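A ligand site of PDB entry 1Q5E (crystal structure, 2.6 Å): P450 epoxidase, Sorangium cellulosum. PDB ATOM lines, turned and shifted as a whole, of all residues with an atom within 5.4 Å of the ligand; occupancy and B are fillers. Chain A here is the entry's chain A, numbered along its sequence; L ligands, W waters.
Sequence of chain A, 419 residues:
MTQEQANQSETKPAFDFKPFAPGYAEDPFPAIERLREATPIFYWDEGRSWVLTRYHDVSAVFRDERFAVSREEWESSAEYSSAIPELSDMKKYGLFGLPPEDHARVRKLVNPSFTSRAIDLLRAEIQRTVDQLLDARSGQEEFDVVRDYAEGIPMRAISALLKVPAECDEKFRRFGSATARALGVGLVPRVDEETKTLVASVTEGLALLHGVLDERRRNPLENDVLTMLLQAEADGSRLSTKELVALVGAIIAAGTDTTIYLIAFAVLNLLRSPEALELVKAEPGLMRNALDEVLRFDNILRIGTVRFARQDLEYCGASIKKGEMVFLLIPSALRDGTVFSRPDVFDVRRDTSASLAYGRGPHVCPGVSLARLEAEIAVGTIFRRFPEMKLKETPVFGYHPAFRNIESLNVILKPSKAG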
ATOM      1  N   PHE A  62      36.849 -10.295 -16.517  1.00  0.00           N
ATOM      2  CA  PHE A  62      36.000 -10.841 -15.476  1.00  0.00           C
ATOM      3  C   PHE A  62      36.820 -11.125 -14.247  1.00  0.00           C
ATOM      4  O   PHE A  62      36.576 -10.528 -13.204  1.00  0.00           O
ATOM      5  CB  PHE A  62      35.375 -12.137 -15.966  1.00  0.00           C
ATOM      6  CG  PHE A  62      33.942 -11.999 -16.412  1.00  0.00           C
ATOM      7  CD1 PHE A  62      33.016 -11.379 -15.614  1.00  0.00           C
ATOM      8  CD2 PHE A  62      33.540 -12.505 -17.638  1.00  0.00           C
ATOM      9  CE1 PHE A  62      31.732 -11.268 -16.035  1.00  0.00           C
ATOM     10  CE2 PHE A  62      32.255 -12.395 -18.059  1.00  0.00           C
ATOM     11  CZ  PHE A  62      31.338 -11.772 -17.263  1.00  0.00           C
ATOM     12  N   VAL A  69      33.580  -2.994 -10.458  1.00  0.00           N
ATOM     13  CA  VAL A  69      32.196  -3.099 -10.868  1.00  0.00           C
ATOM     14  C   VAL A  69      31.471  -1.867 -10.444  1.00  0.00           C
ATOM     15  O   VAL A  69      30.332  -1.661 -10.851  1.00  0.00           O
ATOM     16  CB  VAL A  69      31.499  -4.288 -10.192  1.00  0.00           C
ATOM     17  CG1 VAL A  69      31.948  -5.611 -10.816  1.00  0.00           C
ATOM     18  CG2 VAL A  69      31.792  -4.266  -8.714  1.00  0.00           C
ATOM     19  N   LEU A  95      25.628  -5.878  -3.618  1.00  0.00           N
ATOM     20  CA  LEU A  95      26.695  -6.713  -4.132  1.00  0.00           C
ATOM     21  C   LEU A  95      27.641  -5.974  -5.117  1.00  0.00           C
ATOM     22  O   LEU A  95      28.776  -6.401  -5.312  1.00  0.00           O
ATOM     23  CB  LEU A  95      26.100  -7.977  -4.750  1.00  0.00           C
ATOM     24  CG  LEU A  95      25.601  -9.060  -3.768  1.00  0.00           C
ATOM     25  CD1 LEU A  95      26.604  -9.390  -2.692  1.00  0.00           C
ATOM     26  CD2 LEU A  95      24.313  -8.635  -3.100  1.00  0.00           C
ATOM     27  N   PHE A  96      27.196  -4.870  -5.723  1.00  0.00           N
ATOM     28  CA  PHE A  96      28.007  -4.123  -6.684  1.00  0.00           C
ATOM     29  C   PHE A  96      28.559  -2.840  -6.102  1.00  0.00           C
ATOM     30  O   PHE A  96      29.170  -2.030  -6.814  1.00  0.00           O
ATOM     31  CB  PHE A  96      27.201  -3.798  -7.953  1.00  0.00           C
ATOM     32  CG  PHE A  96      27.219  -4.907  -8.953  1.00  0.00           C
ATOM     33  CD1 PHE A  96      26.907  -6.212  -8.571  1.00  0.00           C
ATOM     34  CD2 PHE A  96      27.593  -4.678 -10.278  1.00  0.00           C
ATOM     35  CE1 PHE A  96      26.922  -7.250  -9.486  1.00  0.00           C
ATOM     36  CE2 PHE A  96      27.606  -5.723 -11.214  1.00  0.00           C
ATOM     37  CZ  PHE A  96      27.292  -7.007 -10.812  1.00  0.00           C
ATOM     38  N   HIS A 103      32.801  -7.829  -0.131  1.00  0.00           N
ATOM     39  CA  HIS A 103      32.012  -8.666  -1.025  1.00  0.00           C
ATOM     40  C   HIS A 103      32.339 -10.161  -0.859  1.00  0.00           C
ATOM     41  O   HIS A 103      31.444 -11.013  -0.878  1.00  0.00           O
ATOM     42  CB  HIS A 103      32.219  -8.187  -2.444  1.00  0.00           C
ATOM     43  CG  HIS A 103      31.627  -9.080  -3.479  1.00  0.00           C
ATOM     44  ND1 HIS A 103      32.233 -10.241  -3.885  1.00  0.00           N
ATOM     45  CD2 HIS A 103      30.523  -8.934  -4.235  1.00  0.00           C
ATOM     46  CE1 HIS A 103      31.512 -10.789  -4.851  1.00  0.00           C
ATOM     47  NE2 HIS A 103      30.469 -10.019  -5.079  1.00  0.00           N
ATOM     48  N   ARG A 107      29.259 -13.010   0.258  1.00  0.00           N
ATOM     49  CA  ARG A 107      29.105 -14.127  -0.660  1.00  0.00           C
ATOM     50  C   ARG A 107      29.232 -15.476   0.039  1.00  0.00           C
ATOM     51  O   ARG A 107      28.327 -16.294  -0.043  1.00  0.00           O
ATOM     52  CB  ARG A 107      30.167 -14.073  -1.758  1.00  0.00           C
ATOM     53  CG  ARG A 107      29.853 -13.162  -2.941  1.00  0.00           C
ATOM     54  CD  ARG A 107      28.471 -13.353  -3.521  1.00  0.00           C
ATOM     55  NE  ARG A 107      28.330 -14.586  -4.308  1.00  0.00           N
ATOM     56  CZ  ARG A 107      28.494 -14.681  -5.635  1.00  0.00           C
ATOM     57  NH1 ARG A 107      28.818 -13.639  -6.376  1.00  0.00           N
ATOM     58  NH2 ARG A 107      28.298 -15.850  -6.235  1.00  0.00           N
ATOM     59  N   PHE A 114      22.415 -21.408  -1.662  1.00  0.00           N
ATOM     60  CA  PHE A 114      22.145 -21.520  -3.091  1.00  0.00           C
ATOM     61  C   PHE A 114      22.726 -22.771  -3.805  1.00  0.00           C
ATOM     62  O   PHE A 114      22.688 -22.855  -5.017  1.00  0.00           O
ATOM     63  CB  PHE A 114      22.578 -20.238  -3.809  1.00  0.00           C
ATOM     64  CG  PHE A 114      21.587 -19.108  -3.714  1.00  0.00           C
ATOM     65  CD1 PHE A 114      21.751 -18.090  -2.766  1.00  0.00           C
ATOM     66  CD2 PHE A 114      20.473 -19.073  -4.559  1.00  0.00           C
ATOM     67  CE1 PHE A 114      20.812 -17.064  -2.648  1.00  0.00           C
ATOM     68  CE2 PHE A 114      19.542 -18.059  -4.471  1.00  0.00           C
ATOM     69  CZ  PHE A 114      19.700 -17.057  -3.521  1.00  0.00           C
ATOM     70  N   ILE A 158      11.553 -17.493  -5.614  1.00  0.00           N
ATOM     71  CA  ILE A 158      12.264 -16.699  -4.640  1.00  0.00           C
ATOM     72  C   ILE A 158      11.409 -16.504  -3.380  1.00  0.00           C
ATOM     73  O   ILE A 158      11.910 -16.636  -2.243  1.00  0.00           O
ATOM     74  CB  ILE A 158      12.692 -15.368  -5.266  1.00  0.00           C
ATOM     75  CG1 ILE A 158      13.548 -15.643  -6.516  1.00  0.00           C
ATOM     76  CG2 ILE A 158      13.461 -14.515  -4.291  1.00  0.00           C
ATOM     77  CD1 ILE A 158      13.758 -14.447  -7.365  1.00  0.00           C
ATOM     78  N   ALA A 250      18.675  -7.046  -4.059  1.00  0.00           N
ATOM     79  CA  ALA A 250      19.498  -7.447  -5.213  1.00  0.00           C
ATOM     80  C   ALA A 250      19.065  -8.809  -5.778  1.00  0.00           C
ATOM     81  O   ALA A 250      18.719  -8.922  -6.941  1.00  0.00           O
ATOM     82  CB  ALA A 250      20.982  -7.521  -4.800  1.00  0.00           C
ATOM     83  N   ILE A 251      19.090  -9.821  -4.928  1.00  0.00           N
ATOM     84  CA  ILE A 251      18.586 -11.124  -5.231  1.00  0.00           C
ATOM     85  C   ILE A 251      17.237 -11.122  -5.975  1.00  0.00           C
ATOM     86  O   ILE A 251      17.115 -11.740  -7.038  1.00  0.00           O
ATOM     87  CB  ILE A 251      18.436 -11.901  -3.920  1.00  0.00           C
ATOM     88  CG1 ILE A 251      19.801 -12.117  -3.272  1.00  0.00           C
ATOM     89  CG2 ILE A 251      17.710 -13.219  -4.139  1.00  0.00           C
ATOM     90  CD1 ILE A 251      19.707 -12.575  -1.780  1.00  0.00           C
ATOM     91  N   ALA A 254      17.693  -9.255  -9.341  1.00  0.00           N
ATOM     92  CA  ALA A 254      18.622  -9.925 -10.246  1.00  0.00           C
ATOM     93  C   ALA A 254      18.102 -11.258 -10.789  1.00  0.00           C
ATOM     94  O   ALA A 254      18.568 -11.747 -11.840  1.00  0.00           O
ATOM     95  CB  ALA A 254      19.964 -10.125  -9.587  1.00  0.00           C
ATOM     96  N   GLY A 255      17.135 -11.853 -10.107  1.00  0.00           N
ATOM     97  CA  GLY A 255      16.645 -13.136 -10.586  1.00  0.00           C
ATOM     98  C   GLY A 255      15.180 -13.131 -10.942  1.00  0.00           C
ATOM     99  O   GLY A 255      14.489 -14.131 -10.755  1.00  0.00           O
ATOM    100  N   THR A 258      15.568 -12.057 -15.548  1.00  0.00           N
ATOM    101  CA  THR A 258      16.497 -13.022 -16.140  1.00  0.00           C
ATOM    102  C   THR A 258      15.804 -14.361 -16.322  1.00  0.00           C
ATOM    103  O   THR A 258      15.856 -14.942 -17.411  1.00  0.00           O
ATOM    104  CB  THR A 258      17.750 -13.226 -15.287  1.00  0.00           C
ATOM    105  OG1 THR A 258      17.342 -13.508 -13.939  1.00  0.00           O
ATOM    106  CG2 THR A 258      18.606 -11.960 -15.232  1.00  0.00           C
ATOM    107  N   THR A 259      15.154 -14.870 -15.290  1.00  0.00           N
ATOM    108  CA  THR A 259      14.676 -16.220 -15.402  1.00  0.00           C
ATOM    109  C   THR A 259      13.520 -16.231 -16.374  1.00  0.00           C
ATOM    110  O   THR A 259      13.341 -17.174 -17.128  1.00  0.00           O
ATOM    111  CB  THR A 259      14.213 -16.728 -14.044  1.00  0.00           C
ATOM    112  OG1 THR A 259      15.301 -16.706 -13.089  1.00  0.00           O
ATOM    113  CG2 THR A 259      13.729 -18.204 -14.143  1.00  0.00           C
ATOM    114  N   LEU A 262      14.874 -16.586 -19.780  1.00  0.00           N
ATOM    115  CA  LEU A 262      15.500 -17.874 -20.084  1.00  0.00           C
ATOM    116  C   LEU A 262      14.403 -18.788 -20.539  1.00  0.00           C
ATOM    117  O   LEU A 262      14.530 -19.438 -21.553  1.00  0.00           O
ATOM    118  CB  LEU A 262      16.223 -18.490 -18.884  1.00  0.00           C
ATOM    119  CG  LEU A 262      16.679 -19.955 -18.994  1.00  0.00           C
ATOM    120  CD1 LEU A 262      17.805 -20.236 -19.990  1.00  0.00           C
ATOM    121  CD2 LEU A 262      17.129 -20.402 -17.614  1.00  0.00           C
ATOM    122  N   LEU A 295      21.287 -20.170 -23.562  1.00  0.00           N
ATOM    123  CA  LEU A 295      21.963 -18.932 -23.222  1.00  0.00           C
ATOM    124  C   LEU A 295      23.197 -18.764 -24.024  1.00  0.00           C
ATOM    125  O   LEU A 295      23.617 -17.630 -24.239  1.00  0.00           O
ATOM    126  CB  LEU A 295      22.334 -18.882 -21.738  1.00  0.00           C
ATOM    127  CG  LEU A 295      21.134 -18.744 -20.774  1.00  0.00           C
ATOM    128  CD1 LEU A 295      21.595 -18.605 -19.301  1.00  0.00           C
ATOM    129  CD2 LEU A 295      20.206 -17.570 -21.173  1.00  0.00           C
ATOM    130  N   ILE A 300      20.336 -13.727 -23.415  1.00  0.00           N
ATOM    131  CA  ILE A 300      19.217 -12.895 -23.071  1.00  0.00           C
ATOM    132  C   ILE A 300      19.616 -11.426 -23.042  1.00  0.00           C
ATOM    133  O   ILE A 300      18.741 -10.556 -23.132  1.00  0.00           O
ATOM    134  CB  ILE A 300      18.646 -13.300 -21.697  1.00  0.00           C
ATOM    135  CG1 ILE A 300      19.684 -13.117 -20.610  1.00  0.00           C
ATOM    136  CG2 ILE A 300      18.135 -14.747 -21.728  1.00  0.00           C
ATOM    137  CD1 ILE A 300      19.130 -13.130 -19.216  1.00  0.00           C
ATOM    138  N   THR A 305      27.764  -7.039 -19.642  1.00  0.00           N
ATOM    139  CA  THR A 305      27.977  -6.722 -18.239  1.00  0.00           C
ATOM    140  C   THR A 305      29.007  -5.565 -18.190  1.00  0.00           C
ATOM    141  O   THR A 305      29.808  -5.412 -19.137  1.00  0.00           O
ATOM    142  CB  THR A 305      28.461  -8.008 -17.505  1.00  0.00           C
ATOM    143  OG1 THR A 305      28.459  -7.784 -16.082  1.00  0.00           O
ATOM    144  CG2 THR A 305      29.903  -8.324 -17.874  1.00  0.00           C
ATOM    145  N   ARG A 307      32.040  -3.068 -16.412  1.00  0.00           N
ATOM    146  CA  ARG A 307      33.215  -2.941 -15.569  1.00  0.00           C
ATOM    147  C   ARG A 307      33.825  -1.540 -15.742  1.00  0.00           C
ATOM    148  O   ARG A 307      33.971  -1.065 -16.877  1.00  0.00           O
ATOM    149  CB  ARG A 307      34.261  -3.988 -15.986  1.00  0.00           C
ATOM    150  CG  ARG A 307      34.520  -5.080 -14.952  1.00  0.00           C
ATOM    151  CD  ARG A 307      33.409  -6.135 -14.896  1.00  0.00           C
ATOM    152  NE  ARG A 307      33.662  -7.119 -13.858  1.00  0.00           N
ATOM    153  CZ  ARG A 307      32.744  -7.881 -13.315  1.00  0.00           C
ATOM    154  NH1 ARG A 307      31.485  -7.779 -13.726  1.00  0.00           N
ATOM    155  NH2 ARG A 307      33.087  -8.760 -12.376  1.00  0.00           N
ATOM    156  N   ILE A 330      28.567  -9.640 -24.352  1.00  0.00           N
ATOM    157  CA  ILE A 330      28.320 -11.066 -24.072  1.00  0.00           C
ATOM    158  C   ILE A 330      27.593 -11.841 -25.165  1.00  0.00           C
ATOM    159  O   ILE A 330      27.891 -13.010 -25.372  1.00  0.00           O
ATOM    160  CB  ILE A 330      27.657 -11.261 -22.674  1.00  0.00           C
ATOM    161  CG1 ILE A 330      28.661 -10.838 -21.603  1.00  0.00           C
ATOM    162  CG2 ILE A 330      27.294 -12.731 -22.458  1.00  0.00           C
ATOM    163  CD1 ILE A 330      28.094 -10.599 -20.267  1.00  0.00           C
ATOM    164  N   LEU A 356      29.706 -18.095 -20.654  1.00  0.00           N
ATOM    165  CA  LEU A 356      29.929 -17.070 -19.665  1.00  0.00           C
ATOM    166  C   LEU A 356      28.594 -16.485 -19.303  1.00  0.00           C
ATOM    167  O   LEU A 356      28.532 -15.523 -18.571  1.00  0.00           O
ATOM    168  CB  LEU A 356      30.791 -15.941 -20.269  1.00  0.00           C
ATOM    169  CG  LEU A 356      32.170 -16.330 -20.796  1.00  0.00           C
ATOM    170  CD1 LEU A 356      32.981 -15.144 -21.205  1.00  0.00           C
ATOM    171  CD2 LEU A 356      32.912 -17.107 -19.773  1.00  0.00           C
ATOM    172  N   ALA A 357      27.501 -17.039 -19.851  1.00  0.00           N
ATOM    173  CA  ALA A 357      26.134 -16.653 -19.433  1.00  0.00           C
ATOM    174  C   ALA A 357      26.009 -16.286 -17.964  1.00  0.00           C
ATOM    175  O   ALA A 357      25.359 -15.297 -17.645  1.00  0.00           O
ATOM    176  CB  ALA A 357      25.099 -17.743 -19.749  1.00  0.00           C
ATOM    177  N   TYR A 358      26.559 -17.104 -17.071  1.00  0.00           N
ATOM    178  CA  TYR A 358      26.428 -16.789 -15.650  1.00  0.00           C
ATOM    179  C   TYR A 358      27.712 -16.214 -15.066  1.00  0.00           C
ATOM    180  O   TYR A 358      27.897 -16.210 -13.848  1.00  0.00           O
ATOM    181  CB  TYR A 358      25.960 -17.993 -14.842  1.00  0.00           C
ATOM    182  CG  TYR A 358      24.649 -18.605 -15.290  1.00  0.00           C
ATOM    183  CD1 TYR A 358      24.619 -19.720 -16.159  1.00  0.00           C
ATOM    184  CD2 TYR A 358      23.429 -18.079 -14.846  1.00  0.00           C
ATOM    185  CE1 TYR A 358      23.413 -20.299 -16.563  1.00  0.00           C
ATOM    186  CE2 TYR A 358      22.209 -18.639 -15.241  1.00  0.00           C
ATOM    187  CZ  TYR A 358      22.212 -19.739 -16.080  1.00  0.00           C
ATOM    188  OH  TYR A 358      21.022 -20.276 -16.453  1.00  0.00           O
ATOM    189  N   GLY A 359      28.560 -15.700 -15.932  1.00  0.00           N
ATOM    190  CA  GLY A 359      29.716 -14.952 -15.504  1.00  0.00           C
ATOM    191  C   GLY A 359      30.885 -15.766 -14.994  1.00  0.00           C
ATOM    192  O   GLY A 359      30.873 -17.018 -15.013  1.00  0.00           O
ATOM    193  N   ARG A 360      31.898 -15.048 -14.532  1.00  0.00           N
ATOM    194  CA  ARG A 360      33.104 -15.647 -14.037  1.00  0.00           C
ATOM    195  C   ARG A 360      33.627 -14.802 -12.873  1.00  0.00           C
ATOM    196  O   ARG A 360      33.217 -13.646 -12.718  1.00  0.00           O
ATOM    197  CB  ARG A 360      34.151 -15.685 -15.171  1.00  0.00           C
ATOM    198  CG  ARG A 360      33.891 -16.740 -16.231  1.00  0.00           C
ATOM    199  CD  ARG A 360      34.222 -18.078 -15.712  1.00  0.00           C
ATOM    200  NE  ARG A 360      34.237 -19.092 -16.764  1.00  0.00           N
ATOM    201  CZ  ARG A 360      33.145 -19.566 -17.307  1.00  0.00           C
ATOM    202  NH1 ARG A 360      31.962 -19.109 -16.932  1.00  0.00           N
ATOM    203  NH2 ARG A 360      33.243 -20.509 -18.212  1.00  0.00           N
ATOM    204  N   PRO A 362      34.717 -13.632  -8.796  1.00  0.00           N
ATOM    205  CA  PRO A 362      33.996 -13.460  -7.530  1.00  0.00           C
ATOM    206  C   PRO A 362      32.510 -13.173  -7.605  1.00  0.00           C
ATOM    207  O   PRO A 362      31.848 -13.610  -6.703  1.00  0.00           O
ATOM    208  CB  PRO A 362      34.765 -12.349  -6.815  1.00  0.00           C
ATOM    209  CG  PRO A 362      35.771 -11.821  -7.826  1.00  0.00           C
ATOM    210  CD  PRO A 362      35.968 -12.825  -8.847  1.00  0.00           C
ATOM    211  N   HIS A 363      31.993 -12.498  -8.636  1.00  0.00           N
ATOM    212  CA  HIS A 363      30.575 -12.178  -8.696  1.00  0.00           C
ATOM    213  C   HIS A 363      29.797 -13.188  -9.542  1.00  0.00           C
ATOM    214  O   HIS A 363      28.669 -12.906  -9.954  1.00  0.00           O
ATOM    215  CB  HIS A 363      30.319 -10.798  -9.309  1.00  0.00           C
ATOM    216  CG  HIS A 363      31.101  -9.705  -8.660  1.00  0.00           C
ATOM    217  ND1 HIS A 363      30.572  -8.919  -7.644  1.00  0.00           N
ATOM    218  CD2 HIS A 363      32.371  -9.271  -8.845  1.00  0.00           C
ATOM    219  CE1 HIS A 363      31.479  -8.045  -7.247  1.00  0.00           C
ATOM    220  NE2 HIS A 363      32.576  -8.250  -7.954  1.00  0.00           N
ATOM    221  N   VAL A 364      30.367 -14.360  -9.812  1.00  0.00           N
ATOM    222  CA  VAL A 364      29.666 -15.320 -10.688  1.00  0.00           C
ATOM    223  C   VAL A 364      28.243 -15.491 -10.111  1.00  0.00           C
ATOM    224  O   VAL A 364      28.021 -15.358  -8.926  1.00  0.00           O
ATOM    225  CB  VAL A 364      30.420 -16.695 -10.768  1.00  0.00           C
ATOM    226  CG1 VAL A 364      30.614 -17.311  -9.307  1.00  0.00           C
ATOM    227  CG2 VAL A 364      29.695 -17.698 -11.602  1.00  0.00           C
ATOM    228  N   CYS A 365      27.268 -15.778 -10.948  1.00  0.00           N
ATOM    229  CA  CYS A 365      25.901 -15.831 -10.472  1.00  0.00           C
ATOM    230  C   CYS A 365      25.647 -16.895  -9.390  1.00  0.00           C
ATOM    231  O   CYS A 365      25.822 -18.082  -9.603  1.00  0.00           O
ATOM    232  CB  CYS A 365      24.968 -16.044 -11.649  1.00  0.00           C
ATOM    233  SG  CYS A 365      23.227 -16.054 -11.258  1.00  0.00           S
ATOM    234  N   PRO A 366      25.190 -16.450  -8.239  1.00  0.00           N
ATOM    235  CA  PRO A 366      24.832 -17.351  -7.144  1.00  0.00           C
ATOM    236  C   PRO A 366      23.447 -18.021  -7.398  1.00  0.00           C
ATOM    237  O   PRO A 366      23.085 -18.956  -6.712  1.00  0.00           O
ATOM    238  CB  PRO A 366      24.772 -16.394  -5.967  1.00  0.00           C
ATOM    239  CG  PRO A 366      24.158 -15.121  -6.627  1.00  0.00           C
ATOM    240  CD  PRO A 366      24.947 -15.026  -7.885  1.00  0.00           C
ATOM    241  N   GLY A 367      22.691 -17.519  -8.373  1.00  0.00           N
ATOM    242  CA  GLY A 367      21.368 -18.026  -8.687  1.00  0.00           C
ATOM    243  C   GLY A 367      21.330 -19.053  -9.816  1.00  0.00           C
ATOM    244  O   GLY A 367      20.279 -19.511 -10.230  1.00  0.00           O
ATOM    245  N   VAL A 368      22.494 -19.462 -10.283  1.00  0.00           N
ATOM    246  CA  VAL A 368      22.538 -20.307 -11.447  1.00  0.00           C
ATOM    247  C   VAL A 368      21.731 -21.562 -11.281  1.00  0.00           C
ATOM    248  O   VAL A 368      20.906 -21.869 -12.129  1.00  0.00           O
ATOM    249  CB  VAL A 368      24.024 -20.633 -11.874  1.00  0.00           C
ATOM    250  CG1 VAL A 368      24.835 -21.203 -10.698  1.00  0.00           C
ATOM    251  CG2 VAL A 368      24.025 -21.605 -13.055  1.00  0.00           C
ATOM    252  N   LEU A 370      19.283 -22.381  -9.233  1.00  0.00           N
ATOM    253  CA  LEU A 370      17.867 -22.077  -9.077  1.00  0.00           C
ATOM    254  C   LEU A 370      17.262 -21.773 -10.424  1.00  0.00           C
ATOM    255  O   LEU A 370      16.187 -22.289 -10.768  1.00  0.00           O
ATOM    256  CB  LEU A 370      17.733 -20.837  -8.176  1.00  0.00           C
ATOM    257  CG  LEU A 370      16.309 -20.347  -7.867  1.00  0.00           C
ATOM    258  CD1 LEU A 370      15.594 -21.296  -6.951  1.00  0.00           C
ATOM    259  CD2 LEU A 370      16.350 -18.985  -7.260  1.00  0.00           C
ATOM    260  N   ALA A 371      17.930 -20.897 -11.185  1.00  0.00           N
ATOM    261  CA  ALA A 371      17.496 -20.578 -12.549  1.00  0.00           C
ATOM    262  C   ALA A 371      17.340 -21.850 -13.411  1.00  0.00           C
ATOM    263  O   ALA A 371      16.331 -22.008 -14.138  1.00  0.00           O
ATOM    264  CB  ALA A 371      18.454 -19.606 -13.199  1.00  0.00           C
ATOM    265  N   GLU A 374      14.259 -24.029 -12.102  1.00  0.00           N
ATOM    266  CA  GLU A 374      13.023 -23.416 -12.571  1.00  0.00           C
ATOM    267  C   GLU A 374      12.744 -23.698 -14.056  1.00  0.00           C
ATOM    268  O   GLU A 374      11.637 -24.148 -14.425  1.00  0.00           O
ATOM    269  CB  GLU A 374      13.062 -21.882 -12.351  1.00  0.00           C
ATOM    270  CG  GLU A 374      12.755 -21.371 -10.926  1.00  0.00           C
ATOM    271  CD  GLU A 374      13.033 -19.869 -10.770  1.00  0.00           C
ATOM    272  OE1 GLU A 374      12.250 -19.087 -11.332  1.00  0.00           O
ATOM    273  OE2 GLU A 374      14.018 -19.410 -10.092  1.00  0.00           O
HETATM  274  C1  LIG L   1      24.994 -12.158 -11.084  1.00  0.00           C
HETATM  275  C2  LIG L   1      22.951 -13.963 -15.076  1.00  0.00           C
HETATM  276  C3  LIG L   1      19.454 -15.829 -12.295  1.00  0.00           C
HETATM  277  C4  LIG L   1      21.168 -13.522  -8.520  1.00  0.00           C
HETATM  278  C5  LIG L   1      24.796 -12.581 -12.392  1.00  0.00           C
HETATM  279  C6  LIG L   1      25.763 -12.377 -13.449  1.00  0.00           C
HETATM  280  C7  LIG L   1      25.209 -12.866 -14.562  1.00  0.00           C
HETATM  281  C8  LIG L   1      23.890 -13.408 -14.229  1.00  0.00           C
HETATM  282  C9  LIG L   1      25.883 -12.858 -15.941  1.00  0.00           C
HETATM  283  C10 LIG L   1      27.171 -11.729 -13.271  1.00  0.00           C
HETATM  284  C11 LIG L   1      27.299 -10.288 -13.775  1.00  0.00           C
HETATM  285  C12 LIG L   1      28.718  -9.799 -13.535  1.00  0.00           C
HETATM  286  O1  LIG L   1      29.022  -9.140 -12.513  1.00  0.00           O
HETATM  287  O2  LIG L   1      29.602 -10.049 -14.382  1.00  0.00           O
HETATM  288  C13 LIG L   1      21.801 -14.602 -14.647  1.00  0.00           C
HETATM  289  C14 LIG L   1      20.890 -15.347 -15.501  1.00  0.00           C
HETATM  290  C15 LIG L   1      19.929 -15.846 -14.715  1.00  0.00           C
HETATM  291  C16 LIG L   1      20.227 -15.456 -13.366  1.00  0.00           C
HETATM  292  C17 LIG L   1      21.006 -15.489 -17.040  1.00  0.00           C
HETATM  293  C18 LIG L   1      18.736 -16.713 -15.111  1.00  0.00           C
HETATM  294  C19 LIG L   1      18.562 -17.241 -16.327  1.00  0.00           C
HETATM  295  C20 LIG L   1      19.626 -15.434 -11.002  1.00  0.00           C
HETATM  296  C21 LIG L   1      18.778 -15.784  -9.847  1.00  0.00           C
HETATM  297  C22 LIG L   1      19.283 -15.117  -8.803  1.00  0.00           C
HETATM  298  C23 LIG L   1      20.426 -14.363  -9.278  1.00  0.00           C
HETATM  299  C24 LIG L   1      17.557 -16.721  -9.877  1.00  0.00           C
HETATM  300  C25 LIG L   1      18.840 -15.081  -7.367  1.00  0.00           C
HETATM  301  C26 LIG L   1      17.867 -15.886  -6.899  1.00  0.00           C
HETATM  302  C27 LIG L   1      22.319 -12.898  -8.906  1.00  0.00           C
HETATM  303  C28 LIG L   1      22.993 -12.018  -8.007  1.00  0.00           C
HETATM  304  C29 LIG L   1      24.235 -11.549  -8.742  1.00  0.00           C
HETATM  305  C30 LIG L   1      24.120 -12.213 -10.056  1.00  0.00           C
HETATM  306  C31 LIG L   1      22.511 -11.684  -6.589  1.00  0.00           C
HETATM  307  C32 LIG L   1      25.284 -10.568  -8.115  1.00  0.00           C
HETATM  308  C33 LIG L   1      26.657 -11.252  -7.963  1.00  0.00           C
HETATM  309  C34 LIG L   1      27.558 -10.584  -6.933  1.00  0.00           C
HETATM  310  O3  LIG L   1      27.512 -10.997  -5.739  1.00  0.00           O
HETATM  311  O4  LIG L   1      28.308  -9.627  -7.258  1.00  0.00           O
HETATM  312  N1  LIG L   1      23.663 -13.234 -12.900  1.00  0.00           N
HETATM  313  N2  LIG L   1      21.377 -14.691 -13.339  1.00  0.00           N
HETATM  314  N3  LIG L   1      20.629 -14.579 -10.622  1.00  0.00           N
HETATM  315  N4  LIG L   1      23.017 -13.017 -10.111  1.00  0.00           N
HETATM  316 FE1  LIG L   1      22.251 -14.052 -11.714  1.00  0.00          FE
HETATM  317  O   HOH W   1      14.248 -16.557  -9.708  1.00  0.00           O
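O of Tyr 358 lies within hydrogen-bond range of N of Cys 365 (3.0 Å). The side-chain hydroxyl of Thr 258 is in hydrogen-bond range of the backbone carbonyl oxygen of Ala 254 (3.0 Å). NH1 of Arg 107 sits at hydrogen-bond distance from O of Pro 362, 3.0 Å away. A ring nitrogen (ND1) of His 363 lies within hydrogen-bond range of a ring nitrogen (NE2) of His 103 (2.8 Å). SG of Cys 365 sits close to N of Val 368, at 3.6 Å. The backbone carbonyl oxygen (O) of Val 364 is in hydrogen-bond range of the guanidinium group (NH2) of Arg 107 (2.7 Å). SG of Cys 365 lies close to N of Gly 367, at 3.3 Å.
The side-chain hydroxyl of Thr 305 is in hydrogen-bond range of an oxygen (O2) of the ligand. A ring nitrogen (ND1) of His 363 sits at hydrogen-bond distance from an oxygen (O4) of the ligand. The guanidinium group of Arg 307 lies within salt-bridge range of an oxygen (O2) of the ligand, at 3.0 Å. An oxygen (O3) of the ligand lies within salt-bridge range of the guanidinium group (NH1) of Arg 107 (3.0 Å). SG of Cys 365 binds FE1 of the ligand (2.3 Å). An oxygen (O4) of the ligand lies within hydrogen-bond range of a ring nitrogen (NE2) of His 103 (3.1 Å).
Water W1 lies within hydrogen-bond range of O of Gly 255 and OE2 of Glu 374.
Phe 62 touches the ligand. Leu 95 touches the ligand (CG to O3, 3.4 Å). Phe 96 touches the ligand. Phe 114 touches the ligand (CE2 to C26, 3.7 Å). Ile 251 touches the ligand (O to C25, 3.8 Å). CB of Ala 254 touches C27 of the ligand, 3.7 Å away. CA of Gly 255 touches C21 of the ligand (3.5 Å). CB of Thr 258 touches C15 of the ligand (3.5 Å). OG1 of Thr 259 touches C24 of the ligand, at 3.9 Å. Leu 262 touches the ligand. Leu 295 touches the ligand. Ile 300 touches the ligand. Ala 357 touches the ligand. Tyr 358 touches the ligand. Gly 359 touches the ligand (N to C9, 3.9 Å). CD of Pro 366 touches C27 of the ligand, 3.5 Å away. Gly 367 touches the ligand (CA to C22, 3.6 Å). Leu 370 touches the ligand. CB of Ala 371 touches C18 of the ligand, 3.5 Å away. Hydrophobic or aromatic side chains within 4 Å of the ligand: Phe 62, Leu 95, Phe 96, His 103, Phe 114, Ile 251, Ala 254, Leu 262, Leu 295, Ile 300, Tyr 358, His 363, Pro 366, Leu 370 and Ala 371. The nearest printed residue that does not touch the ligand is Ile 158 (4.3 Å).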
